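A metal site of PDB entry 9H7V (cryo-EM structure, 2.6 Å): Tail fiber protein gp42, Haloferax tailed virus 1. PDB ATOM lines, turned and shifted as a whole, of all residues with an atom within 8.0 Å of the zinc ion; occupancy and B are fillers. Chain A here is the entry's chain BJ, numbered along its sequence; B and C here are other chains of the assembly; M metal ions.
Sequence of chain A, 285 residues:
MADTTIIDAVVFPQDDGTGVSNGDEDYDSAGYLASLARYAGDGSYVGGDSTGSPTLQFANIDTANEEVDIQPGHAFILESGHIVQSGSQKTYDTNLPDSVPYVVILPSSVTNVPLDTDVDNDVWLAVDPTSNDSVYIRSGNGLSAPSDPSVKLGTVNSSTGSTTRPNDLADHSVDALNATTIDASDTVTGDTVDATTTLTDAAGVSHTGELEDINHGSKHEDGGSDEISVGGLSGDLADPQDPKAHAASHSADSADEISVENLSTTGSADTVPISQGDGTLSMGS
NE2 of His 216 of chain B binds the zinc ion (1.8 Å).
NE2 of His 216 of chain A is bound to the zinc ion (1.9 Å).
A ring nitrogen (NE2) of His 220 of chain A binds the zinc ion, at 1.9 Å.
His 216 of chain C touches the zinc ion (NE2 to ZN, 3.3 Å).
Within 4 Å of the zinc ion: His 216 of chain A, His 220 of chain A, His 216 of chain B and His 216 of chain C.
Along chain A the residues within 4 Å of the zinc ion span positions 216 to 220.
A ring nitrogen (ND1) of His 216 of chain B lies within hydrogen-bond range of the backbone carbonyl oxygen (O) of Asp 213 of chain B, at 2.7 Å.
NE2 of His 216 of chain C sits close to NE2 of His 216 of chain A.
The backbone NH (N) of His 216 of chain B sits at hydrogen-bond distance from the side-chain carboxylate (OD2) of Asp 226 of chain A, 3.1 Å away.
The backbone NH (N) of His 216 of chain A lies within hydrogen-bond range of the side-chain carboxylate (OD2) of Asp 226 of chain C (3.1 Å).
The backbone carbonyl oxygen (O) of Asp 213 of chain C sits at hydrogen-bond distance from a ring nitrogen (ND1) of His 216 of chain C.
A ring nitrogen (ND1) of His 220 of chain A is in hydrogen-bond range of the backbone carbonyl oxygen (O) of Asp 226 of chain A (2.8 Å).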
ATOM      1  N   GLU A 212     -15.136 -23.784 -10.111  1.00  0.00           N
ATOM      2  CA  GLU A 212     -14.758 -22.814 -11.131  1.00  0.00           C
ATOM      3  C   GLU A 212     -13.421 -23.168 -11.771  1.00  0.00           C
ATOM      4  O   GLU A 212     -12.462 -23.522 -11.067  1.00  0.00           O
ATOM      5  CB  GLU A 212     -14.723 -21.398 -10.546  1.00  0.00           C
ATOM      6  CG  GLU A 212     -16.093 -20.851 -10.171  1.00  0.00           C
ATOM      7  CD  GLU A 212     -16.968 -20.320 -11.297  1.00  0.00           C
ATOM      8  OE1 GLU A 212     -17.053 -20.980 -12.360  1.00  0.00           O
ATOM      9  OE2 GLU A 212     -17.561 -19.244 -11.112  1.00  0.00           O
ATOM     10  N   ASP A 213     -13.365 -23.065 -13.108  1.00  0.00           N
ATOM     11  CA  ASP A 213     -12.175 -23.285 -13.924  1.00  0.00           C
ATOM     12  C   ASP A 213     -11.288 -22.035 -13.887  1.00  0.00           C
ATOM     13  O   ASP A 213     -11.739 -20.974 -13.463  1.00  0.00           O
ATOM     14  CB  ASP A 213     -12.528 -23.498 -15.400  1.00  0.00           C
ATOM     15  CG  ASP A 213     -13.535 -24.607 -15.672  1.00  0.00           C
ATOM     16  OD1 ASP A 213     -13.219 -25.773 -15.364  1.00  0.00           O
ATOM     17  OD2 ASP A 213     -14.618 -24.299 -16.199  1.00  0.00           O
ATOM     18  N   HIS A 216     -11.705 -17.652 -15.890  1.00  0.00           N
ATOM     19  CA  HIS A 216     -13.139 -17.525 -15.669  1.00  0.00           C
ATOM     20  C   HIS A 216     -13.568 -16.055 -15.609  1.00  0.00           C
ATOM     21  O   HIS A 216     -14.758 -15.767 -15.687  1.00  0.00           O
ATOM     22  CB  HIS A 216     -13.551 -18.292 -14.398  1.00  0.00           C
ATOM     23  CG  HIS A 216     -13.337 -17.524 -13.131  1.00  0.00           C
ATOM     24  ND1 HIS A 216     -12.095 -17.044 -12.772  1.00  0.00           N
ATOM     25  CD2 HIS A 216     -14.187 -17.160 -12.155  1.00  0.00           C
ATOM     26  CE1 HIS A 216     -12.195 -16.412 -11.623  1.00  0.00           C
ATOM     27  NE2 HIS A 216     -13.469 -16.458 -11.223  1.00  0.00           N
ATOM     28  N   GLY A 217     -12.588 -15.143 -15.460  1.00  0.00           N
ATOM     29  CA  GLY A 217     -12.802 -13.733 -15.164  1.00  0.00           C
ATOM     30  C   GLY A 217     -13.847 -13.045 -16.039  1.00  0.00           C
ATOM     31  O   GLY A 217     -14.530 -12.129 -15.590  1.00  0.00           O
ATOM     32  N   SER A 218     -13.963 -13.531 -17.287  1.00  0.00           N
ATOM     33  CA  SER A 218     -14.927 -13.100 -18.301  1.00  0.00           C
ATOM     34  C   SER A 218     -16.330 -12.902 -17.712  1.00  0.00           C
ATOM     35  O   SER A 218     -17.009 -11.942 -18.067  1.00  0.00           O
ATOM     36  CB  SER A 218     -14.939 -14.073 -19.447  1.00  0.00           C
ATOM     37  OG  SER A 218     -15.911 -13.711 -20.412  1.00  0.00           O
ATOM     38  N   LYS A 219     -16.746 -13.813 -16.814  1.00  0.00           N
ATOM     39  CA  LYS A 219     -18.101 -13.872 -16.300  1.00  0.00           C
ATOM     40  C   LYS A 219     -18.418 -12.682 -15.385  1.00  0.00           C
ATOM     41  O   LYS A 219     -19.578 -12.299 -15.252  1.00  0.00           O
ATOM     42  CB  LYS A 219     -18.389 -15.231 -15.656  1.00  0.00           C
ATOM     43  CG  LYS A 219     -17.788 -15.470 -14.275  1.00  0.00           C
ATOM     44  CD  LYS A 219     -17.773 -16.929 -13.855  1.00  0.00           C
ATOM     45  CE  LYS A 219     -19.153 -17.546 -13.719  1.00  0.00           C
ATOM     46  NZ  LYS A 219     -19.077 -19.013 -13.472  1.00  0.00           N
ATOM     47  N   HIS A 220     -17.380 -12.087 -14.762  1.00  0.00           N
ATOM     48  CA  HIS A 220     -17.564 -11.020 -13.786  1.00  0.00           C
ATOM     49  C   HIS A 220     -17.833  -9.671 -14.472  1.00  0.00           C
ATOM     50  O   HIS A 220     -18.214  -8.711 -13.807  1.00  0.00           O
ATOM     51  CB  HIS A 220     -16.382 -10.955 -12.800  1.00  0.00           C
ATOM     52  CG  HIS A 220     -16.205 -12.155 -11.930  1.00  0.00           C
ATOM     53  ND1 HIS A 220     -17.166 -12.582 -11.043  1.00  0.00           N
ATOM     54  CD2 HIS A 220     -15.166 -13.012 -11.804  1.00  0.00           C
ATOM     55  CE1 HIS A 220     -16.743 -13.663 -10.413  1.00  0.00           C
ATOM     56  NE2 HIS A 220     -15.514 -13.936 -10.860  1.00  0.00           N
ATOM     57  N   SER A 225     -22.697 -13.867 -15.704  1.00  0.00           N
ATOM     58  CA  SER A 225     -23.170 -14.354 -14.412  1.00  0.00           C
ATOM     59  C   SER A 225     -22.118 -14.060 -13.342  1.00  0.00           C
ATOM     60  O   SER A 225     -20.926 -14.203 -13.603  1.00  0.00           O
ATOM     61  CB  SER A 225     -23.521 -15.821 -14.477  1.00  0.00           C
ATOM     62  OG  SER A 225     -22.399 -16.593 -14.879  1.00  0.00           O
ATOM     63  N   ASP A 226     -22.585 -13.653 -12.148  1.00  0.00           N
ATOM     64  CA  ASP A 226     -21.756 -13.301 -11.002  1.00  0.00           C
ATOM     65  C   ASP A 226     -21.015 -11.982 -11.257  1.00  0.00           C
ATOM     66  O   ASP A 226     -19.872 -11.808 -10.816  1.00  0.00           O
ATOM     67  CB  ASP A 226     -20.882 -14.464 -10.512  1.00  0.00           C
ATOM     68  CG  ASP A 226     -20.364 -14.330  -9.097  1.00  0.00           C
ATOM     69  OD1 ASP A 226     -20.953 -13.557  -8.307  1.00  0.00           O
ATOM     70  OD2 ASP A 226     -19.363 -15.007  -8.774  1.00  0.00           O
ATOM     71  N   ILE A 228     -20.027  -8.326 -10.518  1.00  0.00           N
ATOM     72  CA  ILE A 228     -19.795  -7.654  -9.241  1.00  0.00           C
ATOM     73  C   ILE A 228     -20.200  -6.175  -9.349  1.00  0.00           C
ATOM     74  O   ILE A 228     -20.126  -5.587 -10.428  1.00  0.00           O
ATOM     75  CB  ILE A 228     -18.341  -7.824  -8.740  1.00  0.00           C
ATOM     76  CG1 ILE A 228     -17.304  -7.161  -9.667  1.00  0.00           C
ATOM     77  CG2 ILE A 228     -18.023  -9.293  -8.484  1.00  0.00           C
ATOM     78  CD1 ILE A 228     -15.934  -6.965  -9.047  1.00  0.00           C
ATOM     79  N   GLU B 212     -13.213 -22.626  -5.240  1.00  0.00           N
ATOM     80  CA  GLU B 212     -14.267 -21.628  -5.302  1.00  0.00           C
ATOM     81  C   GLU B 212     -15.451 -22.120  -6.137  1.00  0.00           C
ATOM     82  O   GLU B 212     -15.274 -22.586  -7.255  1.00  0.00           O
ATOM     83  CB  GLU B 212     -13.739 -20.293  -5.835  1.00  0.00           C
ATOM     84  CG  GLU B 212     -12.845 -19.550  -4.848  1.00  0.00           C
ATOM     85  CD  GLU B 212     -13.519 -18.778  -3.717  1.00  0.00           C
ATOM     86  OE1 GLU B 212     -14.599 -19.204  -3.258  1.00  0.00           O
ATOM     87  OE2 GLU B 212     -12.954 -17.751  -3.300  1.00  0.00           O
ATOM     88  N   ASP B 213     -16.661 -21.970  -5.568  1.00  0.00           N
ATOM     89  CA  ASP B 213     -17.929 -22.269  -6.212  1.00  0.00           C
ATOM     90  C   ASP B 213     -18.254 -21.197  -7.247  1.00  0.00           C
ATOM     91  O   ASP B 213     -17.556 -20.195  -7.349  1.00  0.00           O
ATOM     92  CB  ASP B 213     -19.088 -22.264  -5.205  1.00  0.00           C
ATOM     93  CG  ASP B 213     -18.810 -22.935  -3.877  1.00  0.00           C
ATOM     94  OD1 ASP B 213     -18.920 -24.170  -3.811  1.00  0.00           O
ATOM     95  OD2 ASP B 213     -18.490 -22.208  -2.908  1.00  0.00           O
ATOM     96  N   ILE B 214     -19.346 -21.403  -8.002  1.00  0.00           N
ATOM     97  CA  ILE B 214     -20.054 -20.327  -8.690  1.00  0.00           C
ATOM     98  C   ILE B 214     -20.644 -19.395  -7.633  1.00  0.00           C
ATOM     99  O   ILE B 214     -20.850 -19.801  -6.490  1.00  0.00           O
ATOM    100  CB  ILE B 214     -21.139 -20.870  -9.647  1.00  0.00           C
ATOM    101  CG1 ILE B 214     -22.209 -21.694  -8.926  1.00  0.00           C
ATOM    102  CG2 ILE B 214     -20.515 -21.635 -10.808  1.00  0.00           C
ATOM    103  CD1 ILE B 214     -23.562 -21.719  -9.611  1.00  0.00           C
ATOM    104  N   ASN B 215     -20.912 -18.129  -8.031  1.00  0.00           N
ATOM    105  CA  ASN B 215     -21.553 -17.114  -7.205  1.00  0.00           C
ATOM    106  C   ASN B 215     -20.662 -16.686  -6.040  1.00  0.00           C
ATOM    107  O   ASN B 215     -21.157 -16.287  -4.987  1.00  0.00           O
ATOM    108  CB  ASN B 215     -22.976 -17.507  -6.762  1.00  0.00           C
ATOM    109  CG  ASN B 215     -23.887 -17.924  -7.906  1.00  0.00           C
ATOM    110  OD1 ASN B 215     -23.772 -17.437  -9.026  1.00  0.00           O
ATOM    111  ND2 ASN B 215     -24.814 -18.825  -7.618  1.00  0.00           N
ATOM    112  N   HIS B 216     -19.335 -16.739  -6.261  1.00  0.00           N
ATOM    113  CA  HIS B 216     -18.342 -16.368  -5.256  1.00  0.00           C
ATOM    114  C   HIS B 216     -18.140 -14.857  -5.204  1.00  0.00           C
ATOM    115  O   HIS B 216     -17.874 -14.307  -4.131  1.00  0.00           O
ATOM    116  CB  HIS B 216     -17.015 -17.087  -5.538  1.00  0.00           C
ATOM    117  CG  HIS B 216     -16.484 -16.824  -6.907  1.00  0.00           C
ATOM    118  ND1 HIS B 216     -16.831 -17.621  -7.988  1.00  0.00           N
ATOM    119  CD2 HIS B 216     -15.670 -15.864  -7.388  1.00  0.00           C
ATOM    120  CE1 HIS B 216     -16.241 -17.160  -9.075  1.00  0.00           C
ATOM    121  NE2 HIS B 216     -15.521 -16.084  -8.728  1.00  0.00           N
ATOM    122  N   GLY B 217     -18.303 -14.189  -6.360  1.00  0.00           N
ATOM    123  CA  GLY B 217     -17.855 -12.826  -6.628  1.00  0.00           C
ATOM    124  C   GLY B 217     -18.321 -11.775  -5.615  1.00  0.00           C
ATOM    125  O   GLY B 217     -17.695 -10.730  -5.483  1.00  0.00           O
ATOM    126  N   SER B 218     -19.429 -12.077  -4.918  1.00  0.00           N
ATOM    127  CA  SER B 218     -20.004 -11.233  -3.869  1.00  0.00           C
ATOM    128  C   SER B 218     -18.998 -10.937  -2.765  1.00  0.00           C
ATOM    129  O   SER B 218     -19.132  -9.936  -2.062  1.00  0.00           O
ATOM    130  CB  SER B 218     -21.257 -11.869  -3.314  1.00  0.00           C
ATOM    131  OG  SER B 218     -21.890 -11.005  -2.375  1.00  0.00           O
ATOM    132  N   LYS B 219     -17.977 -11.807  -2.629  1.00  0.00           N
ATOM    133  CA  LYS B 219     -16.907 -11.661  -1.661  1.00  0.00           C
ATOM    134  C   LYS B 219     -16.085 -10.402  -1.938  1.00  0.00           C
ATOM    135  O   LYS B 219     -15.606  -9.772  -0.992  1.00  0.00           O
ATOM    136  CB  LYS B 219     -16.041 -12.932  -1.626  1.00  0.00           C
ATOM    137  CG  LYS B 219     -15.182 -13.204  -2.854  1.00  0.00           C
ATOM    138  CD  LYS B 219     -14.457 -14.533  -2.811  1.00  0.00           C
ATOM    139  CE  LYS B 219     -13.320 -14.556  -1.797  1.00  0.00           C
ATOM    140  NZ  LYS B 219     -13.061 -15.930  -1.298  1.00  0.00           N
ATOM    141  N   HIS B 220     -15.937 -10.035  -3.217  1.00  0.00           N
ATOM    142  CA  HIS B 220     -15.058  -8.956  -3.651  1.00  0.00           C
ATOM    143  C   HIS B 220     -15.628  -7.572  -3.295  1.00  0.00           C
ATOM    144  O   HIS B 220     -15.006  -6.564  -3.600  1.00  0.00           O
ATOM    145  CB  HIS B 220     -14.747  -9.056  -5.167  1.00  0.00           C
ATOM    146  CG  HIS B 220     -14.214 -10.361  -5.670  1.00  0.00           C
ATOM    147  ND1 HIS B 220     -13.029 -10.912  -5.236  1.00  0.00           N
ATOM    148  CD2 HIS B 220     -14.692 -11.202  -6.618  1.00  0.00           C
ATOM    149  CE1 HIS B 220     -12.809 -12.051  -5.873  1.00  0.00           C
ATOM    150  NE2 HIS B 220     -13.815 -12.251  -6.725  1.00  0.00           N
ATOM    151  N   GLU C 212      -9.717 -23.216  -9.809  1.00  0.00           N
ATOM    152  CA  GLU C 212      -9.508 -21.934  -9.145  1.00  0.00           C
ATOM    153  C   GLU C 212      -9.571 -22.075  -7.622  1.00  0.00           C
ATOM    154  O   GLU C 212     -10.553 -22.564  -7.068  1.00  0.00           O
ATOM    155  CB  GLU C 212     -10.470 -20.865  -9.654  1.00  0.00           C
ATOM    156  CG  GLU C 212     -10.069 -20.257 -10.990  1.00  0.00           C
ATOM    157  CD  GLU C 212      -8.890 -19.301 -11.046  1.00  0.00           C
ATOM    158  OE1 GLU C 212      -8.092 -19.260 -10.081  1.00  0.00           O
ATOM    159  OE2 GLU C 212      -8.755 -18.592 -12.065  1.00  0.00           O
ATOM    160  N   ASP C 213      -8.495 -21.594  -6.979  1.00  0.00           N
ATOM    161  CA  ASP C 213      -8.311 -21.524  -5.536  1.00  0.00           C
ATOM    162  C   ASP C 213      -9.121 -20.361  -4.973  1.00  0.00           C
ATOM    163  O   ASP C 213      -9.673 -19.565  -5.728  1.00  0.00           O
ATOM    164  CB  ASP C 213      -6.834 -21.310  -5.189  1.00  0.00           C
ATOM    165  CG  ASP C 213      -5.866 -22.061  -6.090  1.00  0.00           C
ATOM    166  OD1 ASP C 213      -5.438 -23.159  -5.680  1.00  0.00           O
ATOM    167  OD2 ASP C 213      -5.539 -21.546  -7.170  1.00  0.00           O
ATOM    168  N   HIS C 216      -8.456 -15.631  -5.569  1.00  0.00           N
ATOM    169  CA  HIS C 216      -7.751 -15.622  -6.852  1.00  0.00           C
ATOM    170  C   HIS C 216      -7.766 -14.238  -7.504  1.00  0.00           C
ATOM    171  O   HIS C 216      -7.043 -14.006  -8.464  1.00  0.00           O
ATOM    172  CB  HIS C 216      -8.362 -16.672  -7.780  1.00  0.00           C
ATOM    173  CG  HIS C 216      -9.844 -16.553  -7.917  1.00  0.00           C
ATOM    174  ND1 HIS C 216     -10.724 -17.428  -7.296  1.00  0.00           N
ATOM    175  CD2 HIS C 216     -10.616 -15.657  -8.567  1.00  0.00           C
ATOM    176  CE1 HIS C 216     -11.963 -17.080  -7.570  1.00  0.00           C
ATOM    177  NE2 HIS C 216     -11.924 -15.997  -8.352  1.00  0.00           N
ATOM    178  N   GLY C 217      -8.573 -13.310  -6.954  1.00  0.00           N
ATOM    179  CA  GLY C 217      -8.899 -12.025  -7.564  1.00  0.00           C
ATOM    180  C   GLY C 217      -7.687 -11.165  -7.936  1.00  0.00           C
ATOM    181  O   GLY C 217      -7.790 -10.320  -8.830  1.00  0.00           O
ATOM    182  N   HIS C 220      -6.722 -10.886 -11.566  1.00  0.00           N
ATOM    183  CA  HIS C 220      -7.613 -10.138 -12.452  1.00  0.00           C
ATOM    184  C   HIS C 220      -7.133  -8.698 -12.661  1.00  0.00           C
ATOM    185  O   HIS C 220      -7.620  -8.024 -13.561  1.00  0.00           O
ATOM    186  CB  HIS C 220      -9.062 -10.149 -11.929  1.00  0.00           C
ATOM    187  CG  HIS C 220      -9.735 -11.479 -11.806  1.00  0.00           C
ATOM    188  ND1 HIS C 220      -9.582 -12.495 -12.730  1.00  0.00           N
ATOM    189  CD2 HIS C 220     -10.631 -11.937 -10.903  1.00  0.00           C
ATOM    190  CE1 HIS C 220     -10.321 -13.537 -12.379  1.00  0.00           C
ATOM    191  NE2 HIS C 220     -10.974 -13.211 -11.254  1.00  0.00           N
ATOM    192  N   ASP C 226      -5.847 -13.629 -17.143  1.00  0.00           N
ATOM    193  CA  ASP C 226      -7.270 -13.592 -16.806  1.00  0.00           C
ATOM    194  C   ASP C 226      -7.649 -12.240 -16.197  1.00  0.00           C
ATOM    195  O   ASP C 226      -8.224 -12.176 -15.113  1.00  0.00           O
ATOM    196  CB  ASP C 226      -7.724 -14.826 -16.014  1.00  0.00           C
ATOM    197  CG  ASP C 226      -9.236 -14.986 -15.919  1.00  0.00           C
ATOM    198  OD1 ASP C 226      -9.940 -14.558 -16.862  1.00  0.00           O
ATOM    199  OD2 ASP C 226      -9.705 -15.539 -14.911  1.00  0.00           O
ATOM    200  N   ILE C 228      -9.820  -8.658 -16.120  1.00  0.00           N
ATOM    201  CA  ILE C 228     -11.231  -8.345 -16.325  1.00  0.00           C
ATOM    202  C   ILE C 228     -11.404  -6.892 -16.788  1.00  0.00           C
ATOM    203  O   ILE C 228     -10.692  -6.007 -16.332  1.00  0.00           O
ATOM    204  CB  ILE C 228     -12.095  -8.676 -15.074  1.00  0.00           C
ATOM    205  CG1 ILE C 228     -11.765  -7.792 -13.863  1.00  0.00           C
ATOM    206  CG2 ILE C 228     -11.995 -10.157 -14.740  1.00  0.00           C
ATOM    207  CD1 ILE C 228     -12.749  -7.909 -12.716  1.00  0.00           C
HETATM  208 ZN    ZN M   1     -14.628 -15.443 -10.175  1.00  0.00          ZN
